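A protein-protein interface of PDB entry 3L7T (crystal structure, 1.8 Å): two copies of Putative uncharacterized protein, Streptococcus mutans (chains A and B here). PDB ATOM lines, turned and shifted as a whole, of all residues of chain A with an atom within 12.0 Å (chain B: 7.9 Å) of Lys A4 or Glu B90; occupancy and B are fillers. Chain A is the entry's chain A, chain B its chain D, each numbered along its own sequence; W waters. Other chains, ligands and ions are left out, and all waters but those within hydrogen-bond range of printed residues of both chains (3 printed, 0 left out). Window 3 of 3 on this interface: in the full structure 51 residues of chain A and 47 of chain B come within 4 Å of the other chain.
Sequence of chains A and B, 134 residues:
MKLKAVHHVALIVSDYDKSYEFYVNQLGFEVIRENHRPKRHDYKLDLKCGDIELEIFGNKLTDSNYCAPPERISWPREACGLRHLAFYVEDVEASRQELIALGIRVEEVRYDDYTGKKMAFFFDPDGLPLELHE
O of Lys A4 lies within hydrogen-bond range of N of Gly B50, at 3.2 Å. The backbone carbonyl oxygen (O) of Tyr B88 lies within hydrogen-bond range of the backbone NH (N) of Lys A4 (3.3 Å). NZ of Lys A4 is in salt-bridge range of OE1 of Glu B90, at 3.3 Å. O of Ala A5 sits at hydrogen-bond distance from N of Tyr B88 (2.8 Å). N of Val A6 is in hydrogen-bond range of SG of Cys B49 (3.6 Å). A ring nitrogen (NE2) of His A7 lies within hydrogen-bond range of a ring nitrogen (ND1) of His B133, 3.3 Å away.
A ring nitrogen (ND1) of His A8 is in hydrogen-bond range of a ring nitrogen (ND1) of His A7 (2.7 Å). NZ of Lys B48 lies within hydrogen-bond range of O of Gly B50, 3.0 Å away. N of His B133 lies within hydrogen-bond range of O of Phe B87 (2.9 Å). The backbone carbonyl oxygen (O) of His B133 sits at hydrogen-bond distance from the backbone NH (N) of Val B89 (2.9 Å).
Among the printed residues, merely in contact across the chains: Ala A5 with Phe B87 (3.3 Å), Ala A5 with Cys B49 (3.6 Å), Leu A3 with Phe B29 (3.6 Å), Leu A3 with Val B89 (3.6 Å), Val A6 with Ile B52 (3.7 Å), Lys A2 with Val B89 (3.8 Å), Ile A52 with Ile B52 (3.8 Å), His A7 with Tyr B88 (3.8 Å), Leu A3 with Phe B87 (3.9 Å), His A8 with His B133 (3.9 Å) and His A7 with Phe B87 (3.9 Å).
Of chain B, only Gly B50, Tyr B88 and Glu B90 come within 4 Å of Lys A4. Of chain A, only Lys A4 comes within 4 Å of Glu B90. Cys B49 touches just these residues of chain A: Ala A5 and Val A6. Of chain A, only Lys A4 (3.2 Å) comes within 4 Å of Gly B50. Printed residues of chain A within 4 Å of Tyr B88: Lys A4, Ala A5 and His A7. Of chain A, only Lys A2 and Leu A3 come within 4 Å of Val B89. No residue of chain A comes within 4 Å of Asp B91. Of the printed residues of chain B, Ala A5 touches Cys B49 (3.6 Å), Phe B87 (3.3 Å) and Tyr B88 (2.8 Å). Printed residues of chain B within 4 Å of Val A6: Cys B49 and Ile B52. The nearest printed residue of chain B that does not touch Lys A2 is Tyr B88 (4.2 Å).
Printed residues of chain A that touch a printed residue of chain B: Lys A2, Leu A3, Lys A4, Ala A5, Val A6, His A7, His A8 and Ile A52. Hydrophobic or aromatic side chains of chain A within 4 Å of the printed part of chain B: Leu A3, Val A6, His A7, His A8 and Ile A52. Of the 18 printed residues of chain B, 9 touch a printed residue of chain A. Hydrophobic or aromatic side chains of chain B that line the printed part of chain A: Phe B29, Ile B52, Phe B87, Tyr B88, Val B89 and His B133. Among the printed residues, 17 pairs touch across the chains.
Ile A52 touches its own counterpart, Ile B52. 2 positions are printed for both chains. Of the 17 pairs that touch across the chains among the printed residues, 1 has its exchanged pair printed and touching as well.
Water W1 lies within hydrogen-bond range of the chain-end carboxylate of Glu B134 (2.5 Å) and a ring nitrogen (NE2) of His A7 (3.1 Å). Water W3 bridges the backbone carbonyl oxygen (O) of Lys A2 (2.8 Å) and the backbone NH (N) of Glu B90 (3.1 Å). Water W2 lies within hydrogen-bond range of N of Val A6 (2.8 Å) and O of Cys B49 (2.9 Å).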
ATOM      1  N   LYS A   2      25.757   2.233 -17.227  1.00  0.00           N
ATOM      2  CA  LYS A   2      25.983   2.481 -18.689  1.00  0.00           C
ATOM      3  C   LYS A   2      26.848   3.720 -18.974  1.00  0.00           C
ATOM      4  O   LYS A   2      26.407   4.714 -19.577  1.00  0.00           O
ATOM      5  CB  LYS A   2      24.657   2.545 -19.444  1.00  0.00           C
ATOM      6  CG  LYS A   2      24.120   1.163 -19.814  1.00  0.00           C
ATOM      7  CD  LYS A   2      22.864   1.256 -20.675  1.00  0.00           C
ATOM      8  CE  LYS A   2      22.723   0.028 -21.565  1.00  0.00           C
ATOM      9  NZ  LYS A   2      21.915   0.330 -22.771  1.00  0.00           N
ATOM     10  N   LEU A   3      28.105   3.629 -18.574  1.00  0.00           N
ATOM     11  CA  LEU A   3      29.022   4.735 -18.763  1.00  0.00           C
ATOM     12  C   LEU A   3      29.663   4.561 -20.149  1.00  0.00           C
ATOM     13  O   LEU A   3      30.591   3.779 -20.316  1.00  0.00           O
ATOM     14  CB  LEU A   3      30.073   4.724 -17.651  1.00  0.00           C
ATOM     15  CG  LEU A   3      29.872   5.482 -16.331  1.00  0.00           C
ATOM     16  CD1 LEU A   3      28.447   5.867 -15.988  1.00  0.00           C
ATOM     17  CD2 LEU A   3      30.581   4.817 -15.147  1.00  0.00           C
ATOM     18  N   LYS A   4      29.129   5.285 -21.131  1.00  0.00           N
ATOM     19  CA  LYS A   4      29.281   4.963 -22.541  1.00  0.00           C
ATOM     20  C   LYS A   4      30.647   5.384 -23.082  1.00  0.00           C
ATOM     21  O   LYS A   4      31.195   4.746 -23.970  1.00  0.00           O
ATOM     22  CB  LYS A   4      28.206   5.686 -23.366  1.00  0.00           C
ATOM     23  CG  LYS A   4      26.784   5.258 -23.070  1.00  0.00           C
ATOM     24  CD  LYS A   4      25.804   6.340 -23.490  1.00  0.00           C
ATOM     25  CE  LYS A   4      25.503   6.270 -24.965  1.00  0.00           C
ATOM     26  NZ  LYS A   4      24.669   7.424 -25.389  1.00  0.00           N
ATOM     27  N   ALA A   5      31.160   6.485 -22.555  1.00  0.00           N
ATOM     28  CA  ALA A   5      32.329   7.142 -23.120  1.00  0.00           C
ATOM     29  C   ALA A   5      32.731   8.227 -22.127  1.00  0.00           C
ATOM     30  O   ALA A   5      32.004   8.501 -21.171  1.00  0.00           O
ATOM     31  CB  ALA A   5      31.994   7.751 -24.492  1.00  0.00           C
ATOM     32  N   VAL A   6      33.958   8.697 -22.248  1.00  0.00           N
ATOM     33  CA  VAL A   6      34.375   9.888 -21.527  1.00  0.00           C
ATOM     34  C   VAL A   6      33.757  11.093 -22.220  1.00  0.00           C
ATOM     35  O   VAL A   6      33.798  11.204 -23.449  1.00  0.00           O
ATOM     36  CB  VAL A   6      35.913  10.002 -21.492  1.00  0.00           C
ATOM     37  CG1 VAL A   6      36.329  11.339 -20.915  1.00  0.00           C
ATOM     38  CG2 VAL A   6      36.455   8.897 -20.623  1.00  0.00           C
ATOM     39  N   HIS A   7      33.203  11.991 -21.424  1.00  0.00           N
ATOM     40  CA  HIS A   7      32.674  13.253 -21.916  1.00  0.00           C
ATOM     41  C   HIS A   7      33.768  14.313 -21.939  1.00  0.00           C
ATOM     42  O   HIS A   7      33.981  14.995 -22.956  1.00  0.00           O
ATOM     43  CB  HIS A   7      31.542  13.718 -21.006  1.00  0.00           C
ATOM     44  CG  HIS A   7      30.920  14.995 -21.468  1.00  0.00           C
ATOM     45  ND1 HIS A   7      31.335  16.224 -21.020  1.00  0.00           N
ATOM     46  CD2 HIS A   7      29.938  15.230 -22.374  1.00  0.00           C
ATOM     47  CE1 HIS A   7      30.654  17.173 -21.652  1.00  0.00           C
ATOM     48  NE2 HIS A   7      29.784  16.590 -22.460  1.00  0.00           N
ATOM     49  N   HIS A   8      34.461  14.448 -20.812  1.00  0.00           N
ATOM     50  CA  HIS A   8      35.584  15.396 -20.727  1.00  0.00           C
ATOM     51  C   HIS A   8      36.544  15.021 -19.605  1.00  0.00           C
ATOM     52  O   HIS A   8      36.210  14.224 -18.705  1.00  0.00           O
ATOM     53  CB  HIS A   8      35.061  16.854 -20.564  1.00  0.00           C
ATOM     54  CG  HIS A   8      34.415  17.135 -19.240  1.00  0.00           C
ATOM     55  ND1 HIS A   8      33.055  17.026 -19.032  1.00  0.00           N
ATOM     56  CD2 HIS A   8      34.932  17.607 -18.080  1.00  0.00           C
ATOM     57  CE1 HIS A   8      32.766  17.413 -17.800  1.00  0.00           C
ATOM     58  NE2 HIS A   8      33.897  17.723 -17.190  1.00  0.00           N
ATOM     59  N   ASP A  51      36.247  13.260 -29.844  1.00  0.00           N
ATOM     60  CA  ASP A  51      34.929  13.283 -29.198  1.00  0.00           C
ATOM     61  C   ASP A  51      34.936  13.649 -27.726  1.00  0.00           C
ATOM     62  O   ASP A  51      33.922  13.562 -27.069  1.00  0.00           O
ATOM     63  CB  ASP A  51      34.200  11.948 -29.352  1.00  0.00           C
ATOM     64  CG  ASP A  51      34.236  11.420 -30.764  1.00  0.00           C
ATOM     65  OD1 ASP A  51      33.883  12.159 -31.719  1.00  0.00           O
ATOM     66  OD2 ASP A  51      34.577  10.224 -30.902  1.00  0.00           O
ATOM     67  N   ILE A  52      36.073  14.065 -27.191  1.00  0.00           N
ATOM     68  CA  ILE A  52      36.151  14.312 -25.768  1.00  0.00           C
ATOM     69  C   ILE A  52      36.577  15.769 -25.653  1.00  0.00           C
ATOM     70  O   ILE A  52      37.412  16.222 -26.433  1.00  0.00           O
ATOM     71  CB  ILE A  52      37.214  13.368 -25.140  1.00  0.00           C
ATOM     72  CG1 ILE A  52      36.635  11.955 -25.045  1.00  0.00           C
ATOM     73  CG2 ILE A  52      37.697  13.876 -23.773  1.00  0.00           C
ATOM     74  CD1 ILE A  52      37.634  10.863 -24.759  1.00  0.00           C
ATOM     75  N   PHE B  29      32.645  -1.241 -15.772  1.00  0.00           N
ATOM     76  CA  PHE B  29      33.577  -1.169 -16.883  1.00  0.00           C
ATOM     77  C   PHE B  29      34.079  -2.545 -17.237  1.00  0.00           C
ATOM     78  O   PHE B  29      34.458  -3.339 -16.366  1.00  0.00           O
ATOM     79  CB  PHE B  29      34.774  -0.253 -16.602  1.00  0.00           C
ATOM     80  CG  PHE B  29      34.420   1.207 -16.587  1.00  0.00           C
ATOM     81  CD1 PHE B  29      33.965   1.842 -17.739  1.00  0.00           C
ATOM     82  CD2 PHE B  29      34.520   1.933 -15.404  1.00  0.00           C
ATOM     83  CE1 PHE B  29      33.659   3.208 -17.729  1.00  0.00           C
ATOM     84  CE2 PHE B  29      34.192   3.285 -15.369  1.00  0.00           C
ATOM     85  CZ  PHE B  29      33.798   3.933 -16.548  1.00  0.00           C
ATOM     86  N   LYS B  48      37.826  -0.627 -20.595  1.00  0.00           N
ATOM     87  CA  LYS B  48      37.323  -0.002 -21.796  1.00  0.00           C
ATOM     88  C   LYS B  48      36.273   1.049 -21.436  1.00  0.00           C
ATOM     89  O   LYS B  48      35.333   0.783 -20.668  1.00  0.00           O
ATOM     90  CB  LYS B  48      36.750  -1.044 -22.773  1.00  0.00           C
ATOM     91  CG  LYS B  48      36.157  -0.436 -24.053  1.00  0.00           C
ATOM     92  CD  LYS B  48      35.881  -1.535 -25.116  1.00  0.00           C
ATOM     93  CE  LYS B  48      35.494  -0.951 -26.475  1.00  0.00           C
ATOM     94  NZ  LYS B  48      34.249  -0.130 -26.411  1.00  0.00           N
ATOM     95  N   CYS B  49      36.443   2.241 -21.993  1.00  0.00           N
ATOM     96  CA  CYS B  49      35.440   3.289 -21.891  1.00  0.00           C
ATOM     97  C   CYS B  49      35.230   3.958 -23.251  1.00  0.00           C
ATOM     98  O   CYS B  49      36.102   4.667 -23.749  1.00  0.00           O
ATOM     99  CB  CYS B  49      35.833   4.331 -20.843  1.00  0.00           C
ATOM    100  SG  CYS B  49      34.507   5.533 -20.627  1.00  0.00           S
ATOM    101  N   GLY B  50      34.142   3.600 -23.932  1.00  0.00           N
ATOM    102  CA  GLY B  50      34.001   3.957 -25.352  1.00  0.00           C
ATOM    103  C   GLY B  50      35.231   3.546 -26.137  1.00  0.00           C
ATOM    104  O   GLY B  50      35.714   2.422 -25.986  1.00  0.00           O
ATOM    105  N   ASP B  51      35.848   4.507 -26.817  1.00  0.00           N
ATOM    106  CA  ASP B  51      37.036   4.239 -27.637  1.00  0.00           C
ATOM    107  C   ASP B  51      38.358   4.619 -26.977  1.00  0.00           C
ATOM    108  O   ASP B  51      39.389   4.716 -27.641  1.00  0.00           O
ATOM    109  CB  ASP B  51      36.920   4.933 -28.985  1.00  0.00           C
ATOM    110  CG  ASP B  51      35.786   4.378 -29.811  1.00  0.00           C
ATOM    111  OD1 ASP B  51      35.610   3.143 -29.778  1.00  0.00           O
ATOM    112  OD2 ASP B  51      35.017   5.175 -30.384  1.00  0.00           O
ATOM    113  N   ILE B  52      38.338   4.809 -25.669  1.00  0.00           N
ATOM    114  CA  ILE B  52      39.593   4.981 -24.958  1.00  0.00           C
ATOM    115  C   ILE B  52      39.733   3.927 -23.873  1.00  0.00           C
ATOM    116  O   ILE B  52      38.771   3.231 -23.557  1.00  0.00           O
ATOM    117  CB  ILE B  52      39.735   6.389 -24.372  1.00  0.00           C
ATOM    118  CG1 ILE B  52      39.035   6.513 -23.030  1.00  0.00           C
ATOM    119  CG2 ILE B  52      39.266   7.465 -25.362  1.00  0.00           C
ATOM    120  CD1 ILE B  52      39.598   7.691 -22.227  1.00  0.00           C
ATOM    121  N   PHE B  87      31.957  11.175 -17.421  1.00  0.00           N
ATOM    122  CA  PHE B  87      31.498  10.162 -18.358  1.00  0.00           C
ATOM    123  C   PHE B  87      30.195  10.615 -18.967  1.00  0.00           C
ATOM    124  O   PHE B  87      29.319  11.137 -18.265  1.00  0.00           O
ATOM    125  CB  PHE B  87      31.262   8.855 -17.597  1.00  0.00           C
ATOM    126  CG  PHE B  87      32.485   8.328 -16.927  1.00  0.00           C
ATOM    127  CD1 PHE B  87      33.526   7.805 -17.687  1.00  0.00           C
ATOM    128  CD2 PHE B  87      32.578   8.291 -15.542  1.00  0.00           C
ATOM    129  CE1 PHE B  87      34.676   7.318 -17.097  1.00  0.00           C
ATOM    130  CE2 PHE B  87      33.736   7.784 -14.920  1.00  0.00           C
ATOM    131  CZ  PHE B  87      34.786   7.314 -15.700  1.00  0.00           C
ATOM    132  N   TYR B  88      30.007  10.268 -20.230  1.00  0.00           N
ATOM    133  CA  TYR B  88      28.813  10.635 -20.958  1.00  0.00           C
ATOM    134  C   TYR B  88      27.750   9.576 -20.703  1.00  0.00           C
ATOM    135  O   TYR B  88      28.049   8.391 -20.753  1.00  0.00           O
ATOM    136  CB  TYR B  88      29.162  10.672 -22.445  1.00  0.00           C
ATOM    137  CG  TYR B  88      28.006  11.024 -23.333  1.00  0.00           C
ATOM    138  CD1 TYR B  88      27.369  12.251 -23.209  1.00  0.00           C
ATOM    139  CD2 TYR B  88      27.595  10.157 -24.335  1.00  0.00           C
ATOM    140  CE1 TYR B  88      26.325  12.595 -24.047  1.00  0.00           C
ATOM    141  CE2 TYR B  88      26.542  10.475 -25.161  1.00  0.00           C
ATOM    142  CZ  TYR B  88      25.922  11.706 -25.023  1.00  0.00           C
ATOM    143  OH  TYR B  88      24.867  12.030 -25.834  1.00  0.00           O
ATOM    144  N   VAL B  89      26.559  10.002 -20.291  1.00  0.00           N
ATOM    145  CA  VAL B  89      25.446   9.064 -20.105  1.00  0.00           C
ATOM    146  C   VAL B  89      24.180   9.619 -20.775  1.00  0.00           C
ATOM    147  O   VAL B  89      24.073  10.830 -21.071  1.00  0.00           O
ATOM    148  CB  VAL B  89      25.137   8.762 -18.612  1.00  0.00           C
ATOM    149  CG1 VAL B  89      26.332   8.091 -17.921  1.00  0.00           C
ATOM    150  CG2 VAL B  89      24.762  10.041 -17.894  1.00  0.00           C
ATOM    151  N   GLU B  90      23.215   8.734 -20.998  1.00  0.00           N
ATOM    152  CA  GLU B  90      21.938   9.153 -21.582  1.00  0.00           C
ATOM    153  C   GLU B  90      20.998   9.809 -20.586  1.00  0.00           C
ATOM    154  O   GLU B  90      20.284  10.745 -20.934  1.00  0.00           O
ATOM    155  CB  GLU B  90      21.248   7.980 -22.255  1.00  0.00           C
ATOM    156  CG  GLU B  90      21.698   7.794 -23.696  1.00  0.00           C
ATOM    157  CD  GLU B  90      21.143   6.521 -24.303  1.00  0.00           C
ATOM    158  OE1 GLU B  90      21.950   5.704 -24.804  1.00  0.00           O
ATOM    159  OE2 GLU B  90      19.907   6.318 -24.220  1.00  0.00           O
ATOM    160  N   ASP B  91      21.075   9.379 -19.333  1.00  0.00           N
ATOM    161  CA  ASP B  91      20.124   9.794 -18.312  1.00  0.00           C
ATOM    162  C   ASP B  91      20.867   9.977 -17.002  1.00  0.00           C
ATOM    163  O   ASP B  91      21.125   9.011 -16.299  1.00  0.00           O
ATOM    164  CB  ASP B  91      19.049   8.706 -18.162  1.00  0.00           C
ATOM    165  CG  ASP B  91      17.834   9.173 -17.376  1.00  0.00           C
ATOM    166  OD1 ASP B  91      17.993   9.916 -16.382  1.00  0.00           O
ATOM    167  OD2 ASP B  91      16.724   8.699 -17.702  1.00  0.00           O
ATOM    168  N   VAL B  92      21.285  11.207 -16.709  1.00  0.00           N
ATOM    169  CA  VAL B  92      21.984  11.479 -15.459  1.00  0.00           C
ATOM    170  C   VAL B  92      21.155  11.052 -14.229  1.00  0.00           C
ATOM    171  O   VAL B  92      21.652  10.385 -13.338  1.00  0.00           O
ATOM    172  CB  VAL B  92      22.389  12.965 -15.361  1.00  0.00           C
ATOM    173  CG1 VAL B  92      22.741  13.352 -13.911  1.00  0.00           C
ATOM    174  CG2 VAL B  92      23.598  13.220 -16.278  1.00  0.00           C
ATOM    175  N   GLU B  93      19.879  11.405 -14.230  1.00  0.00           N
ATOM    176  CA  GLU B  93      18.982  11.060 -13.124  1.00  0.00           C
ATOM    177  C   GLU B  93      18.939   9.543 -12.864  1.00  0.00           C
ATOM    178  O   GLU B  93      19.196   9.103 -11.742  1.00  0.00           O
ATOM    179  CB  GLU B  93      17.587  11.608 -13.408  1.00  0.00           C
ATOM    180  CG  GLU B  93      16.531  11.079 -12.482  1.00  0.00           C
ATOM    181  CD  GLU B  93      16.426  11.893 -11.223  1.00  0.00           C
ATOM    182  OE1 GLU B  93      17.477  12.361 -10.725  1.00  0.00           O
ATOM    183  OE2 GLU B  93      15.286  12.086 -10.745  1.00  0.00           O
ATOM    184  N   ALA B  94      18.753   8.759 -13.928  1.00  0.00           N
ATOM    185  CA  ALA B  94      18.680   7.295 -13.810  1.00  0.00           C
ATOM    186  C   ALA B  94      20.000   6.634 -13.416  1.00  0.00           C
ATOM    187  O   ALA B  94      20.014   5.767 -12.552  1.00  0.00           O
ATOM    188  CB  ALA B  94      18.119   6.672 -15.065  1.00  0.00           C
ATOM    189  N   SER B  95      21.114   7.103 -13.988  1.00  0.00           N
ATOM    190  CA  SER B  95      22.444   6.605 -13.634  1.00  0.00           C
ATOM    191  C   SER B  95      22.780   6.961 -12.198  1.00  0.00           C
ATOM    192  O   SER B  95      23.420   6.191 -11.474  1.00  0.00           O
ATOM    193  CB  SER B  95      23.514   7.205 -14.578  1.00  0.00           C
ATOM    194  OG  SER B  95      23.373   6.713 -15.901  1.00  0.00           O
ATOM    195  N   LYS B 118      22.414  18.163 -18.093  1.00  0.00           N
ATOM    196  CA  LYS B 118      22.401  17.652 -16.723  1.00  0.00           C
ATOM    197  C   LYS B 118      23.728  16.955 -16.394  1.00  0.00           C
ATOM    198  O   LYS B 118      24.379  16.388 -17.276  1.00  0.00           O
ATOM    199  CB  LYS B 118      21.225  16.694 -16.543  1.00  0.00           C
ATOM    200  CG  LYS B 118      19.875  17.421 -16.549  1.00  0.00           C
ATOM    201  CD  LYS B 118      18.724  16.503 -16.946  1.00  0.00           C
ATOM    202  CE  LYS B 118      18.160  15.790 -15.739  1.00  0.00           C
ATOM    203  NZ  LYS B 118      17.177  16.658 -15.034  1.00  0.00           N
ATOM    204  N   HIS B 133      27.434  12.977 -17.052  1.00  0.00           N
ATOM    205  CA  HIS B 133      27.185  14.190 -17.826  1.00  0.00           C
ATOM    206  C   HIS B 133      26.366  13.804 -19.059  1.00  0.00           C
ATOM    207  O   HIS B 133      26.672  12.815 -19.695  1.00  0.00           O
ATOM    208  CB  HIS B 133      28.522  14.796 -18.261  1.00  0.00           C
ATOM    209  CG  HIS B 133      28.416  16.209 -18.727  1.00  0.00           C
ATOM    210  ND1 HIS B 133      27.755  16.560 -19.883  1.00  0.00           N
ATOM    211  CD2 HIS B 133      28.855  17.362 -18.179  1.00  0.00           C
ATOM    212  CE1 HIS B 133      27.883  17.861 -20.079  1.00  0.00           C
ATOM    213  NE2 HIS B 133      28.552  18.370 -19.062  1.00  0.00           N
ATOM    214  N   GLU B 134      25.277  14.520 -19.310  1.00  0.00           N
ATOM    215  CA  GLU B 134      24.428  14.235 -20.465  1.00  0.00           C
ATOM    216  C   GLU B 134      24.876  14.998 -21.698  1.00  0.00           C
ATOM    217  O   GLU B 134      25.947  15.637 -21.749  1.00  0.00           O
ATOM    218  CB  GLU B 134      22.952  14.550 -20.169  1.00  0.00           C
ATOM    219  CG  GLU B 134      22.167  13.380 -19.636  1.00  0.00           C
ATOM    220  CD  GLU B 134      20.742  13.768 -19.236  1.00  0.00           C
ATOM    221  OE1 GLU B 134      20.160  14.643 -19.898  1.00  0.00           O
ATOM    222  OE2 GLU B 134      20.250  13.281 -18.207  1.00  0.00           O
ATOM    223  OXT GLU B 134      24.156  14.931 -22.693  1.00  0.00           O
HETATM  224  O   HOH W   1      27.035  16.461 -23.803  1.00  0.00           O
HETATM  225  O   HOH W   2      35.584   7.477 -24.204  1.00  0.00           O
HETATM  226  O   HOH W   3      24.000   5.769 -20.504  1.00  0.00           O
